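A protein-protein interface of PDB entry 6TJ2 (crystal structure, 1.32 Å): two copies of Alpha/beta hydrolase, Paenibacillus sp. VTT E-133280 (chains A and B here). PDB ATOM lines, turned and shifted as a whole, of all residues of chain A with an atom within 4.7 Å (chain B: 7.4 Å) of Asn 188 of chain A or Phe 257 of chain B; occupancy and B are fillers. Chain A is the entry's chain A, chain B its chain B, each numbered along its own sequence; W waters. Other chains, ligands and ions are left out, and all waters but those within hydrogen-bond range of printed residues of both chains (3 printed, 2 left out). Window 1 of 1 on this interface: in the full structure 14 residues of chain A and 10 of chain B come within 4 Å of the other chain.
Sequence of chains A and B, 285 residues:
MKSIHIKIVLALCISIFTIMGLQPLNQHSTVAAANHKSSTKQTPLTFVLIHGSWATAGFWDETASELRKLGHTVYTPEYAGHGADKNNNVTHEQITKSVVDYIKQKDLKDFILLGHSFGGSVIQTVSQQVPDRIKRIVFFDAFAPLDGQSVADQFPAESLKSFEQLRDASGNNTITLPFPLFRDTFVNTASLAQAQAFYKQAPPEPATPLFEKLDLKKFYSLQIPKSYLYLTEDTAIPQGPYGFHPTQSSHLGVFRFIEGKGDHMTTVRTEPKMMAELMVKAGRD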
ATOM      1  N   ARG A 183     -15.638  -1.360   3.184  1.00  0.00           N
ATOM      2  CA  ARG A 183     -15.689  -2.510   2.252  1.00  0.00           C
ATOM      3  C   ARG A 183     -15.076  -3.728   2.932  1.00  0.00           C
ATOM      4  O   ARG A 183     -15.571  -4.850   2.752  1.00  0.00           O
ATOM      5  CB  ARG A 183     -15.015  -2.113   0.935  1.00  0.00           C
ATOM      6  CG  ARG A 183     -15.279  -3.126  -0.190  1.00  0.00           C
ATOM      7  CD  ARG A 183     -14.236  -4.229  -0.185  1.00  0.00           C
ATOM      8  NE  ARG A 183     -14.564  -5.252  -1.165  1.00  0.00           N
ATOM      9  CZ  ARG A 183     -15.408  -6.256  -0.986  1.00  0.00           C
ATOM     10  NH1 ARG A 183     -16.085  -6.418   0.135  1.00  0.00           N
ATOM     11  NH2 ARG A 183     -15.634  -7.117  -1.950  1.00  0.00           N
ATOM     12  N   ASP A 184     -13.937  -3.534   3.554  1.00  0.00           N
ATOM     13  CA  ASP A 184     -13.142  -4.654   4.088  1.00  0.00           C
ATOM     14  C   ASP A 184     -13.511  -5.034   5.524  1.00  0.00           C
ATOM     15  O   ASP A 184     -13.129  -6.149   5.895  1.00  0.00           O
ATOM     16  CB  ASP A 184     -11.640  -4.453   3.864  1.00  0.00           C
ATOM     17  CG  ASP A 184     -11.194  -4.780   2.443  1.00  0.00           C
ATOM     18  OD1 ASP A 184     -11.908  -5.437   1.716  1.00  0.00           O
ATOM     19  OD2 ASP A 184     -10.018  -4.448   2.187  1.00  0.00           O
ATOM     20  N   THR A 185     -14.219  -4.217   6.290  1.00  0.00           N
ATOM     21  CA  THR A 185     -14.506  -4.570   7.693  1.00  0.00           C
ATOM     22  C   THR A 185     -15.959  -4.488   8.064  1.00  0.00           C
ATOM     23  O   THR A 185     -16.291  -5.070   9.117  1.00  0.00           O
ATOM     24  CB  THR A 185     -13.670  -3.780   8.699  1.00  0.00           C
ATOM     25  OG1 THR A 185     -14.127  -2.434   8.793  1.00  0.00           O
ATOM     26  CG2 THR A 185     -12.203  -3.824   8.345  1.00  0.00           C
ATOM     27  N   PHE A 186     -16.842  -3.863   7.289  1.00  0.00           N
ATOM     28  CA  PHE A 186     -18.290  -3.847   7.555  1.00  0.00           C
ATOM     29  C   PHE A 186     -19.038  -4.804   6.638  1.00  0.00           C
ATOM     30  O   PHE A 186     -20.055  -5.380   7.006  1.00  0.00           O
ATOM     31  CB  PHE A 186     -18.856  -2.427   7.425  1.00  0.00           C
ATOM     32  CG  PHE A 186     -18.571  -1.539   8.608  1.00  0.00           C
ATOM     33  CD1 PHE A 186     -19.637  -0.968   9.282  1.00  0.00           C
ATOM     34  CD2 PHE A 186     -17.301  -1.220   9.040  1.00  0.00           C
ATOM     35  CE1 PHE A 186     -19.434  -0.142  10.382  1.00  0.00           C
ATOM     36  CE2 PHE A 186     -17.099  -0.364  10.121  1.00  0.00           C
ATOM     37  CZ  PHE A 186     -18.189   0.147  10.798  1.00  0.00           C
ATOM     38  N   VAL A 187     -18.576  -4.877   5.380  1.00  0.00           N
ATOM     39  CA  VAL A 187     -19.211  -5.739   4.351  1.00  0.00           C
ATOM     40  C   VAL A 187     -18.163  -6.666   3.706  1.00  0.00           C
ATOM     41  O   VAL A 187     -18.134  -6.889   2.475  1.00  0.00           O
ATOM     42  CB  VAL A 187     -19.983  -4.885   3.327  1.00  0.00           C
ATOM     43  CG1 VAL A 187     -21.176  -4.203   3.976  1.00  0.00           C
ATOM     44  CG2 VAL A 187     -19.134  -3.859   2.625  1.00  0.00           C
ATOM     45  N   ASN A 188     -17.254  -7.197   4.508  1.00  0.00           N
ATOM     46  CA  ASN A 188     -16.162  -8.061   4.039  1.00  0.00           C
ATOM     47  C   ASN A 188     -16.665  -9.255   3.250  1.00  0.00           C
ATOM     48  O   ASN A 188     -15.904  -9.663   2.324  1.00  0.00           O
ATOM     49  CB  ASN A 188     -15.302  -8.515   5.237  1.00  0.00           C
ATOM     50  CG  ASN A 188     -16.029  -8.845   6.521  1.00  0.00           C
ATOM     51  OD1 ASN A 188     -16.807  -8.040   7.011  1.00  0.00           O
ATOM     52  ND2 ASN A 188     -15.726 -10.009   7.085  1.00  0.00           N
ATOM     53  N   THR A 189     -17.861  -9.763   3.437  1.00  0.00           N
ATOM     54  CA  THR A 189     -18.338 -10.957   2.676  1.00  0.00           C
ATOM     55  C   THR A 189     -19.101 -10.538   1.419  1.00  0.00           C
ATOM     56  O   THR A 189     -19.485 -11.436   0.659  1.00  0.00           O
ATOM     57  CB  THR A 189     -19.190 -11.876   3.558  1.00  0.00           C
ATOM     58  OG1 THR A 189     -20.422 -11.227   3.869  1.00  0.00           O
ATOM     59  CG2 THR A 189     -18.486 -12.243   4.834  1.00  0.00           C
ATOM     60  N   ALA A 190     -19.320  -9.263   1.200  1.00  0.00           N
ATOM     61  CA  ALA A 190     -20.026  -8.778  -0.006  1.00  0.00           C
ATOM     62  C   ALA A 190     -19.092  -8.732  -1.212  1.00  0.00           C
ATOM     63  O   ALA A 190     -17.879  -8.553  -1.070  1.00  0.00           O
ATOM     64  CB  ALA A 190     -20.561  -7.372   0.235  1.00  0.00           C
ATOM     65  N   THR A 232     -20.148 -14.804  12.665  1.00  0.00           N
ATOM     66  CA  THR A 232     -18.721 -15.058  12.976  1.00  0.00           C
ATOM     67  C   THR A 232     -17.740 -14.327  12.054  1.00  0.00           C
ATOM     68  O   THR A 232     -16.559 -14.327  12.407  1.00  0.00           O
ATOM     69  CB  THR A 232     -18.410 -16.547  12.949  1.00  0.00           C
ATOM     70  OG1 THR A 232     -18.537 -17.055  11.624  1.00  0.00           O
ATOM     71  CG2 THR A 232     -19.287 -17.348  13.896  1.00  0.00           C
ATOM     72  N   GLU A 233     -18.185 -13.673  10.980  1.00  0.00           N
ATOM     73  CA  GLU A 233     -17.291 -12.865  10.150  1.00  0.00           C
ATOM     74  C   GLU A 233     -17.559 -11.374  10.422  1.00  0.00           C
ATOM     75  O   GLU A 233     -17.071 -10.532   9.646  1.00  0.00           O
ATOM     76  CB  GLU A 233     -17.427 -13.216   8.674  1.00  0.00           C
ATOM     77  CG  GLU A 233     -16.715 -14.533   8.301  1.00  0.00           C
ATOM     78  CD  GLU A 233     -17.201 -15.086   7.000  1.00  0.00           C
ATOM     79  OE1 GLU A 233     -18.390 -15.456   6.904  1.00  0.00           O
ATOM     80  OE2 GLU A 233     -16.399 -15.172   6.046  1.00  0.00           O
ATOM     81  N   THR A 235     -16.582  -8.081  11.717  1.00  0.00           N
ATOM     82  CA  THR A 235     -15.322  -7.432  12.072  1.00  0.00           C
ATOM     83  C   THR A 235     -15.510  -5.909  12.180  1.00  0.00           C
ATOM     84  O   THR A 235     -14.527  -5.179  12.116  1.00  0.00           O
ATOM     85  CB  THR A 235     -14.267  -7.746  11.029  1.00  0.00           C
ATOM     86  OG1 THR A 235     -14.732  -7.406   9.725  1.00  0.00           O
ATOM     87  CG2 THR A 235     -13.908  -9.203  11.031  1.00  0.00           C
ATOM     88  N   GLN A 239     -11.951  -8.457  15.518  1.00  0.00           N
ATOM     89  CA  GLN A 239     -11.954  -9.664  16.332  1.00  0.00           C
ATOM     90  C   GLN A 239     -10.645  -9.798  17.134  1.00  0.00           C
ATOM     91  O   GLN A 239      -9.608  -9.344  16.684  1.00  0.00           O
ATOM     92  CB  GLN A 239     -12.220 -10.892  15.473  1.00  0.00           C
ATOM     93  CG  GLN A 239     -13.596 -10.793  14.818  1.00  0.00           C
ATOM     94  CD  GLN A 239     -14.094 -11.989  14.072  1.00  0.00           C
ATOM     95  OE1 GLN A 239     -15.215 -11.958  13.454  1.00  0.00           O
ATOM     96  NE2 GLN A 239     -13.372 -13.078  14.088  1.00  0.00           N
ATOM     97  N   ASP A 263     -21.644 -11.145   8.281  1.00  0.00           N
ATOM     98  CA  ASP A 263     -20.816  -9.971   8.650  1.00  0.00           C
ATOM     99  C   ASP A 263     -21.709  -8.829   9.118  1.00  0.00           C
ATOM    100  O   ASP A 263     -22.889  -9.032   9.380  1.00  0.00           O
ATOM    101  CB  ASP A 263     -19.913  -9.610   7.469  1.00  0.00           C
ATOM    102  CG  ASP A 263     -20.690  -9.060   6.302  1.00  0.00           C
ATOM    103  OD1 ASP A 263     -21.900  -8.711   6.477  1.00  0.00           O
ATOM    104  OD2 ASP A 263     -20.051  -8.928   5.200  1.00  0.00           O
ATOM    105  N   ARG B 136      -3.533  -7.101  -4.189  1.00  0.00           N
ATOM    106  CA  ARG B 136      -4.054  -7.461  -2.853  1.00  0.00           C
ATOM    107  C   ARG B 136      -3.164  -8.569  -2.327  1.00  0.00           C
ATOM    108  O   ARG B 136      -2.702  -9.371  -3.126  1.00  0.00           O
ATOM    109  CB  ARG B 136      -5.536  -7.848  -2.932  1.00  0.00           C
ATOM    110  CG  ARG B 136      -6.177  -8.247  -1.618  1.00  0.00           C
ATOM    111  CD  ARG B 136      -7.674  -8.376  -1.712  1.00  0.00           C
ATOM    112  NE  ARG B 136      -8.323  -7.064  -1.696  1.00  0.00           N
ATOM    113  CZ  ARG B 136      -8.706  -6.386  -0.573  1.00  0.00           C
ATOM    114  NH1 ARG B 136      -8.635  -6.828   0.715  1.00  0.00           N
ATOM    115  NH2 ARG B 136      -9.230  -5.186  -0.739  1.00  0.00           N
ATOM    116  N   LYS B 226      -5.129  -5.882   2.247  1.00  0.00           N
ATOM    117  CA  LYS B 226      -4.799  -7.208   2.798  1.00  0.00           C
ATOM    118  C   LYS B 226      -6.105  -7.932   3.133  1.00  0.00           C
ATOM    119  O   LYS B 226      -7.110  -7.329   3.567  1.00  0.00           O
ATOM    120  CB  LYS B 226      -3.950  -7.050   4.058  1.00  0.00           C
ATOM    121  CG  LYS B 226      -2.597  -6.359   3.857  1.00  0.00           C
ATOM    122  CD  LYS B 226      -2.045  -5.810   5.153  1.00  0.00           C
ATOM    123  CE  LYS B 226      -0.901  -4.860   4.941  1.00  0.00           C
ATOM    124  NZ  LYS B 226      -1.403  -3.622   4.299  1.00  0.00           N
ATOM    125  N   SER B 227      -6.080  -9.259   2.985  1.00  0.00           N
ATOM    126  CA  SER B 227      -7.132 -10.155   3.489  1.00  0.00           C
ATOM    127  C   SER B 227      -6.519 -11.289   4.308  1.00  0.00           C
ATOM    128  O   SER B 227      -5.313 -11.576   4.176  1.00  0.00           O
ATOM    129  CB  SER B 227      -7.926 -10.789   2.366  1.00  0.00           C
ATOM    130  OG  SER B 227      -8.490  -9.770   1.534  1.00  0.00           O
ATOM    131  N   TYR B 228      -7.328 -11.838   5.214  1.00  0.00           N
ATOM    132  CA  TYR B 228      -6.920 -13.035   5.976  1.00  0.00           C
ATOM    133  C   TYR B 228      -8.024 -14.039   5.773  1.00  0.00           C
ATOM    134  O   TYR B 228      -9.177 -13.800   6.163  1.00  0.00           O
ATOM    135  CB  TYR B 228      -6.691 -12.703   7.469  1.00  0.00           C
ATOM    136  CG  TYR B 228      -5.826 -13.708   8.168  1.00  0.00           C
ATOM    137  CD1 TYR B 228      -6.323 -14.959   8.540  1.00  0.00           C
ATOM    138  CD2 TYR B 228      -4.482 -13.466   8.388  1.00  0.00           C
ATOM    139  CE1 TYR B 228      -5.507 -15.934   9.104  1.00  0.00           C
ATOM    140  CE2 TYR B 228      -3.641 -14.434   8.907  1.00  0.00           C
ATOM    141  CZ  TYR B 228      -4.162 -15.656   9.274  1.00  0.00           C
ATOM    142  OH  TYR B 228      -3.333 -16.642   9.797  1.00  0.00           O
ATOM    143  N   LEU B 229      -7.623 -15.180   5.247  1.00  0.00           N
ATOM    144  CA  LEU B 229      -8.520 -16.341   4.989  1.00  0.00           C
ATOM    145  C   LEU B 229      -8.184 -17.380   6.041  1.00  0.00           C
ATOM    146  O   LEU B 229      -7.032 -17.834   6.125  1.00  0.00           O
ATOM    147  CB  LEU B 229      -8.299 -16.868   3.580  1.00  0.00           C
ATOM    148  CG  LEU B 229      -9.069 -18.133   3.179  1.00  0.00           C
ATOM    149  CD1 LEU B 229     -10.556 -18.117   3.479  1.00  0.00           C
ATOM    150  CD2 LEU B 229      -8.721 -18.508   1.739  1.00  0.00           C
ATOM    151  N   TYR B 230      -9.129 -17.642   6.921  1.00  0.00           N
ATOM    152  CA  TYR B 230      -8.942 -18.492   8.132  1.00  0.00           C
ATOM    153  C   TYR B 230      -9.888 -19.686   8.083  1.00  0.00           C
ATOM    154  O   TYR B 230     -11.094 -19.516   7.909  1.00  0.00           O
ATOM    155  CB  TYR B 230      -9.245 -17.696   9.371  1.00  0.00           C
ATOM    156  CG  TYR B 230      -9.139 -18.474  10.654  1.00  0.00           C
ATOM    157  CD1 TYR B 230     -10.196 -18.573  11.519  1.00  0.00           C
ATOM    158  CD2 TYR B 230      -7.986 -19.138  10.998  1.00  0.00           C
ATOM    159  CE1 TYR B 230     -10.113 -19.243  12.733  1.00  0.00           C
ATOM    160  CE2 TYR B 230      -7.880 -19.862  12.177  1.00  0.00           C
ATOM    161  CZ  TYR B 230      -8.941 -19.915  13.047  1.00  0.00           C
ATOM    162  OH  TYR B 230      -8.833 -20.589  14.244  1.00  0.00           O
ATOM    163  N   LEU B 231      -9.325 -20.894   8.290  1.00  0.00           N
ATOM    164  CA  LEU B 231     -10.090 -22.144   8.432  1.00  0.00           C
ATOM    165  C   LEU B 231     -10.174 -22.506   9.908  1.00  0.00           C
ATOM    166  O   LEU B 231      -9.128 -22.583  10.591  1.00  0.00           O
ATOM    167  CB  LEU B 231      -9.567 -23.279   7.573  1.00  0.00           C
ATOM    168  CG  LEU B 231      -9.383 -22.942   6.102  1.00  0.00           C
ATOM    169  CD1 LEU B 231      -8.841 -24.158   5.364  1.00  0.00           C
ATOM    170  CD2 LEU B 231     -10.716 -22.523   5.456  1.00  0.00           C
ATOM    171  N   THR B 232     -11.375 -22.746  10.445  1.00  0.00           N
ATOM    172  CA  THR B 232     -11.595 -22.714  11.912  1.00  0.00           C
ATOM    173  C   THR B 232     -11.050 -23.942  12.639  1.00  0.00           C
ATOM    174  O   THR B 232     -10.997 -23.891  13.896  1.00  0.00           O
ATOM    175  CB  THR B 232     -13.051 -22.459  12.299  1.00  0.00           C
ATOM    176  OG1 THR B 232     -13.848 -23.547  11.873  1.00  0.00           O
ATOM    177  CG2 THR B 232     -13.524 -21.156  11.672  1.00  0.00           C
ATOM    178  N   HIS B 245      -5.802 -16.934  14.099  1.00  0.00           N
ATOM    179  CA  HIS B 245      -6.849 -15.886  14.146  1.00  0.00           C
ATOM    180  C   HIS B 245      -7.540 -15.982  15.483  1.00  0.00           C
ATOM    181  O   HIS B 245      -8.012 -17.048  15.839  1.00  0.00           O
ATOM    182  CB  HIS B 245      -7.877 -16.076  13.006  1.00  0.00           C
ATOM    183  CG  HIS B 245      -8.959 -15.044  13.069  1.00  0.00           C
ATOM    184  ND1 HIS B 245      -8.770 -13.742  12.690  1.00  0.00           N
ATOM    185  CD2 HIS B 245     -10.226 -15.148  13.505  1.00  0.00           C
ATOM    186  CE1 HIS B 245      -9.888 -13.073  12.919  1.00  0.00           C
ATOM    187  NE2 HIS B 245     -10.783 -13.897  13.404  1.00  0.00           N
ATOM    188  N   PRO B 246      -7.736 -14.871  16.220  1.00  0.00           N
ATOM    189  CA  PRO B 246      -7.393 -13.513  15.801  1.00  0.00           C
ATOM    190  C   PRO B 246      -5.951 -13.060  16.017  1.00  0.00           C
ATOM    191  O   PRO B 246      -5.644 -11.918  15.660  1.00  0.00           O
ATOM    192  CB  PRO B 246      -8.335 -12.654  16.669  1.00  0.00           C
ATOM    193  CG  PRO B 246      -8.568 -13.519  17.887  1.00  0.00           C
ATOM    194  CD  PRO B 246      -8.541 -14.961  17.437  1.00  0.00           C
ATOM    195  N   SER B 249      -3.678 -12.741  12.484  1.00  0.00           N
ATOM    196  CA  SER B 249      -4.376 -11.835  11.538  1.00  0.00           C
ATOM    197  C   SER B 249      -4.346 -10.401  12.083  1.00  0.00           C
ATOM    198  O   SER B 249      -4.250  -9.460  11.290  1.00  0.00           O
ATOM    199  CB  SER B 249      -5.749 -12.287  11.285  1.00  0.00           C
ATOM    200  OG  SER B 249      -6.476 -12.307  12.496  1.00  0.00           O
ATOM    201  N   VAL B 254      -5.804  -3.246   9.555  1.00  0.00           N
ATOM    202  CA  VAL B 254      -7.089  -3.320   8.814  1.00  0.00           C
ATOM    203  C   VAL B 254      -6.907  -4.363   7.715  1.00  0.00           C
ATOM    204  O   VAL B 254      -5.936  -4.302   6.910  1.00  0.00           O
ATOM    205  CB  VAL B 254      -7.491  -1.960   8.227  1.00  0.00           C
ATOM    206  CG1 VAL B 254      -8.755  -2.026   7.381  1.00  0.00           C
ATOM    207  CG2 VAL B 254      -7.654  -0.919   9.315  1.00  0.00           C
ATOM    208  N   PHE B 255      -7.849  -5.297   7.628  1.00  0.00           N
ATOM    209  CA  PHE B 255      -7.804  -6.364   6.611  1.00  0.00           C
ATOM    210  C   PHE B 255      -9.220  -6.872   6.423  1.00  0.00           C
ATOM    211  O   PHE B 255     -10.065  -6.754   7.335  1.00  0.00           O
ATOM    212  CB  PHE B 255      -6.835  -7.490   7.038  1.00  0.00           C
ATOM    213  CG  PHE B 255      -7.266  -8.273   8.248  1.00  0.00           C
ATOM    214  CD1 PHE B 255      -7.995  -9.436   8.150  1.00  0.00           C
ATOM    215  CD2 PHE B 255      -6.937  -7.843   9.528  1.00  0.00           C
ATOM    216  CE1 PHE B 255      -8.455 -10.095   9.281  1.00  0.00           C
ATOM    217  CE2 PHE B 255      -7.423  -8.498  10.639  1.00  0.00           C
ATOM    218  CZ  PHE B 255      -8.118  -9.654  10.522  1.00  0.00           C
ATOM    219  N   ARG B 256      -9.443  -7.616   5.349  1.00  0.00           N
ATOM    220  CA  ARG B 256     -10.703  -8.294   5.057  1.00  0.00           C
ATOM    221  C   ARG B 256     -10.648  -9.732   5.561  1.00  0.00           C
ATOM    222  O   ARG B 256      -9.841 -10.512   5.094  1.00  0.00           O
ATOM    223  CB  ARG B 256     -10.962  -8.326   3.556  1.00  0.00           C
ATOM    224  CG  ARG B 256     -12.328  -8.924   3.222  1.00  0.00           C
ATOM    225  CD  ARG B 256     -12.482  -9.320   1.758  1.00  0.00           C
ATOM    226  NE  ARG B 256     -12.302  -8.148   0.912  1.00  0.00           N
ATOM    227  CZ  ARG B 256     -12.050  -8.154  -0.382  1.00  0.00           C
ATOM    228  NH1 ARG B 256     -12.041  -9.306  -1.031  1.00  0.00           N
ATOM    229  NH2 ARG B 256     -11.760  -7.024  -0.981  1.00  0.00           N
ATOM    230  N   PHE B 257     -11.469 -10.049   6.569  1.00  0.00           N
ATOM    231  CA  PHE B 257     -11.552 -11.395   7.151  1.00  0.00           C
ATOM    232  C   PHE B 257     -12.523 -12.251   6.353  1.00  0.00           C
ATOM    233  O   PHE B 257     -13.698 -11.853   6.173  1.00  0.00           O
ATOM    234  CB  PHE B 257     -12.015 -11.276   8.592  1.00  0.00           C
ATOM    235  CG  PHE B 257     -12.129 -12.593   9.325  1.00  0.00           C
ATOM    236  CD1 PHE B 257     -11.050 -13.450   9.440  1.00  0.00           C
ATOM    237  CD2 PHE B 257     -13.329 -12.987   9.864  1.00  0.00           C
ATOM    238  CE1 PHE B 257     -11.187 -14.631  10.126  1.00  0.00           C
ATOM    239  CE2 PHE B 257     -13.482 -14.190  10.540  1.00  0.00           C
ATOM    240  CZ  PHE B 257     -12.373 -14.988  10.707  1.00  0.00           C
ATOM    241  N   ILE B 258     -12.093 -13.447   5.949  1.00  0.00           N
ATOM    242  CA  ILE B 258     -12.945 -14.474   5.303  1.00  0.00           C
ATOM    243  C   ILE B 258     -12.726 -15.765   6.068  1.00  0.00           C
ATOM    244  O   ILE B 258     -11.562 -16.186   6.212  1.00  0.00           O
ATOM    245  CB  ILE B 258     -12.598 -14.622   3.819  1.00  0.00           C
ATOM    246  CG1 ILE B 258     -12.879 -13.320   3.050  1.00  0.00           C
ATOM    247  CG2 ILE B 258     -13.373 -15.786   3.198  1.00  0.00           C
ATOM    248  CD1 ILE B 258     -14.348 -12.864   3.029  1.00  0.00           C
ATOM    249  N   GLU B 259     -13.819 -16.370   6.503  1.00  0.00           N
ATOM    250  CA  GLU B 259     -13.755 -17.586   7.319  1.00  0.00           C
ATOM    251  C   GLU B 259     -14.248 -18.780   6.525  1.00  0.00           C
ATOM    252  O   GLU B 259     -15.246 -18.699   5.781  1.00  0.00           O
ATOM    253  CB  GLU B 259     -14.616 -17.403   8.573  1.00  0.00           C
ATOM    254  CG  GLU B 259     -14.598 -18.539   9.606  1.00  0.00           C
ATOM    255  CD  GLU B 259     -15.765 -18.411  10.632  1.00  0.00           C
ATOM    256  OE1 GLU B 259     -16.875 -18.737  10.245  1.00  0.00           O
ATOM    257  OE2 GLU B 259     -15.466 -18.046  11.720  1.00  0.00           O
ATOM    258  N   GLY B 260     -13.634 -19.929   6.707  1.00  0.00           N
ATOM    259  CA  GLY B 260     -14.168 -21.184   6.181  1.00  0.00           C
ATOM    260  C   GLY B 260     -13.932 -22.338   7.143  1.00  0.00           C
ATOM    261  O   GLY B 260     -13.398 -22.141   8.218  1.00  0.00           O
ATOM    262  N   LYS B 281     -13.317 -14.964  -2.654  1.00  0.00           N
ATOM    263  CA  LYS B 281     -13.960 -14.023  -1.706  1.00  0.00           C
ATOM    264  C   LYS B 281     -12.885 -13.194  -0.998  1.00  0.00           C
ATOM    265  O   LYS B 281     -13.092 -12.019  -0.718  1.00  0.00           O
ATOM    266  CB  LYS B 281     -14.752 -14.789  -0.648  1.00  0.00           C
ATOM    267  CG  LYS B 281     -16.110 -15.277  -1.090  1.00  0.00           C
ATOM    268  CD  LYS B 281     -16.823 -16.026   0.050  1.00  0.00           C
ATOM    269  CE  LYS B 281     -17.327 -15.233   1.212  1.00  0.00           C
ATOM    270  NZ  LYS B 281     -18.314 -16.064   1.983  1.00  0.00           N
ATOM    271  N   ALA B 282     -11.707 -13.766  -0.711  1.00  0.00           N
ATOM    272  CA  ALA B 282     -10.628 -13.044  -0.050  1.00  0.00           C
ATOM    273  C   ALA B 282      -9.868 -12.147  -1.025  1.00  0.00           C
ATOM    274  O   ALA B 282      -9.297 -11.123  -0.599  1.00  0.00           O
ATOM    275  CB  ALA B 282      -9.669 -14.038   0.602  1.00  0.00           C
ATOM    276  N   ARG B 284     -10.888 -10.924  -4.306  1.00  0.00           N
ATOM    277  CA  ARG B 284     -11.606 -10.044  -5.235  1.00  0.00           C
ATOM    278  C   ARG B 284     -11.558  -8.604  -4.740  1.00  0.00           C
ATOM    279  O   ARG B 284     -11.348  -8.335  -3.544  1.00  0.00           O
ATOM    280  CB  ARG B 284     -13.058 -10.455  -5.417  1.00  0.00           C
ATOM    281  CG  ARG B 284     -13.888 -10.434  -4.135  1.00  0.00           C
ATOM    282  CD  ARG B 284     -15.238 -11.048  -4.377  1.00  0.00           C
ATOM    283  NE  ARG B 284     -16.059 -11.069  -3.161  1.00  0.00           N
ATOM    284  CZ  ARG B 284     -17.237 -11.615  -3.038  1.00  0.00           C
ATOM    285  NH1 ARG B 284     -17.843 -12.053  -4.112  1.00  0.00           N
ATOM    286  NH2 ARG B 284     -17.838 -11.736  -1.859  1.00  0.00           N
HETATM  287  O   HOH W   1     -12.730  -7.954   8.039  1.00  0.00           O
HETATM  288  O   HOH W   2     -19.712 -15.472   4.509  1.00  0.00           O
HETATM  289  O   HOH W   3     -16.733 -16.965   4.106  1.00  0.00           O
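OD2 of Asp 184 of chain A lies within salt-bridge range of NH2 of Arg 136 of chain B (3.1 Å).
The guanidinium group (NE) of Arg 256 of chain B lies within salt-bridge range of the side-chain carboxylate (OD1) of Asp 184 of chain A (2.9 Å).
ND2 of Asn 188 of chain A lies within hydrogen-bond range of O of Phe 257 of chain B (2.9 Å).
The guanidinium group of Arg 284 of chain B sits at hydrogen-bond distance from the backbone carbonyl oxygen of Thr 189 of chain A (3.0 Å).
O of Ala 190 of chain A lies within hydrogen-bond range of NH2 of Arg 284 of chain B, at 3.3 Å.
The side-chain carboxylate of Glu 259 of chain B lies within hydrogen-bond range of the side-chain hydroxyl of Thr 232 of chain A (2.7 Å).
OE2 of Glu 233 of chain A lies within hydrogen-bond range of N of Glu 259 of chain B.
The side-chain amide nitrogen (NE2) of Gln 239 of chain A lies within hydrogen-bond range of a ring nitrogen (NE2) of His 245 of chain B (2.8 Å).
NH2 of Arg 256 of chain B lies close to NE of Arg 183 of chain A (3.3 Å).
O of Phe 255 of chain B sits close to O of Asp 184 of chain A, 3.4 Å away.
The backbone carbonyl oxygen of Ala 190 of chain A is in hydrogen-bond range of the guanidinium group of Arg 183 of chain A, at 2.8 Å.
The side-chain hydroxyl (OG1) of Thr 189 of chain A is in hydrogen-bond range of the side-chain carboxylate (OD2) of Asp 263 of chain A, 2.7 Å away.
OG of Ser 249 of chain B sits at hydrogen-bond distance from ND1 of His 245 of chain B, 2.7 Å away.
O of Pro 246 of chain B is in hydrogen-bond range of OG of Ser 249 of chain B, 3.3 Å away.
NH1 of Arg 256 of chain B is in hydrogen-bond range of O of Ala 282 of chain B, at 3.3 Å.
Among the printed residues, merely in contact across the chains: Asn 188 of chain A with Arg 256 of chain B, Gln 239 of chain A with Pro 246 of chain B, Glu 233 of chain A with Ile 258 of chain B, Thr 232 of chain A with Phe 257 of chain B, Asn 188 of chain A with Ile 258 of chain B, Thr 235 of chain A with Phe 257 of chain B, Gln 239 of chain A with Phe 257 of chain B, Thr 185 of chain A with Phe 255 of chain B and Glu 233 of chain A with Phe 257 of chain B.
Water W3 lies within hydrogen-bond range of the side-chain carboxylate of Glu 233 of chain A, the side-chain amino group of Lys 281 of chain B and the backbone carbonyl oxygen of Glu 259 of chain B.
Water W1 lies within hydrogen-bond range of the side-chain hydroxyl (OG1) of Thr 235 of chain A (2.7 Å), the backbone carbonyl oxygen (O) of Asp 184 of chain A (2.8 Å), the backbone NH (N) of Phe 257 of chain B (2.9 Å) and the backbone carbonyl oxygen (O) of Phe 255 of chain B (3.0 Å).
Water W2 lies within hydrogen-bond range of OE1 of Glu 233 of chain A and NZ of Lys 281 of chain B.
Asn 188 of chain A touches just these residues of chain B: Arg 256, Phe 257 and Ile 258.
Phe 257 of chain B touches five residues of chain A.
Printed residues of chain B within 4 Å of Asp 184 of chain A: Arg 136, Phe 255 and Arg 256.
Of the printed residues of chain A, Phe 255 of chain B touches Asp 184 (3.4 Å) and Thr 185 (3.8 Å).
Printed residues of chain B within 4 Å of Thr 232 of chain A: Phe 257 (3.6 Å) and Glu 259 (2.7 Å).
Printed residues of chain A within 4 Å of Glu 259 of chain B: Thr 232 (2.7 Å) and Glu 233 (2.9 Å).
Of the printed residues of chain B, Gln 239 of chain A touches His 245 (2.8 Å), Pro 246 (3.5 Å) and Phe 257 (3.7 Å).
The nearest residue of chain A that does not touch Phe 257 of chain B is Asp 184 of chain A (4.3 Å).
The nearest printed residue of chain B that does not touch Gln 239 of chain A is Glu 259 of chain B (5.9 Å).
Printed residues of chain A that touch a printed residue of chain B: Arg 183, Asp 184, Thr 185, Asn 188, Thr 189, Ala 190, Thr 232, Glu 233, Thr 235 and Gln 239.
Printed residues of chain B that touch a printed residue of chain A: Arg 136, His 245, Pro 246, Phe 255, Arg 256, Phe 257, Ile 258, Glu 259 and Arg 284.
Position printed for both chains: 232.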
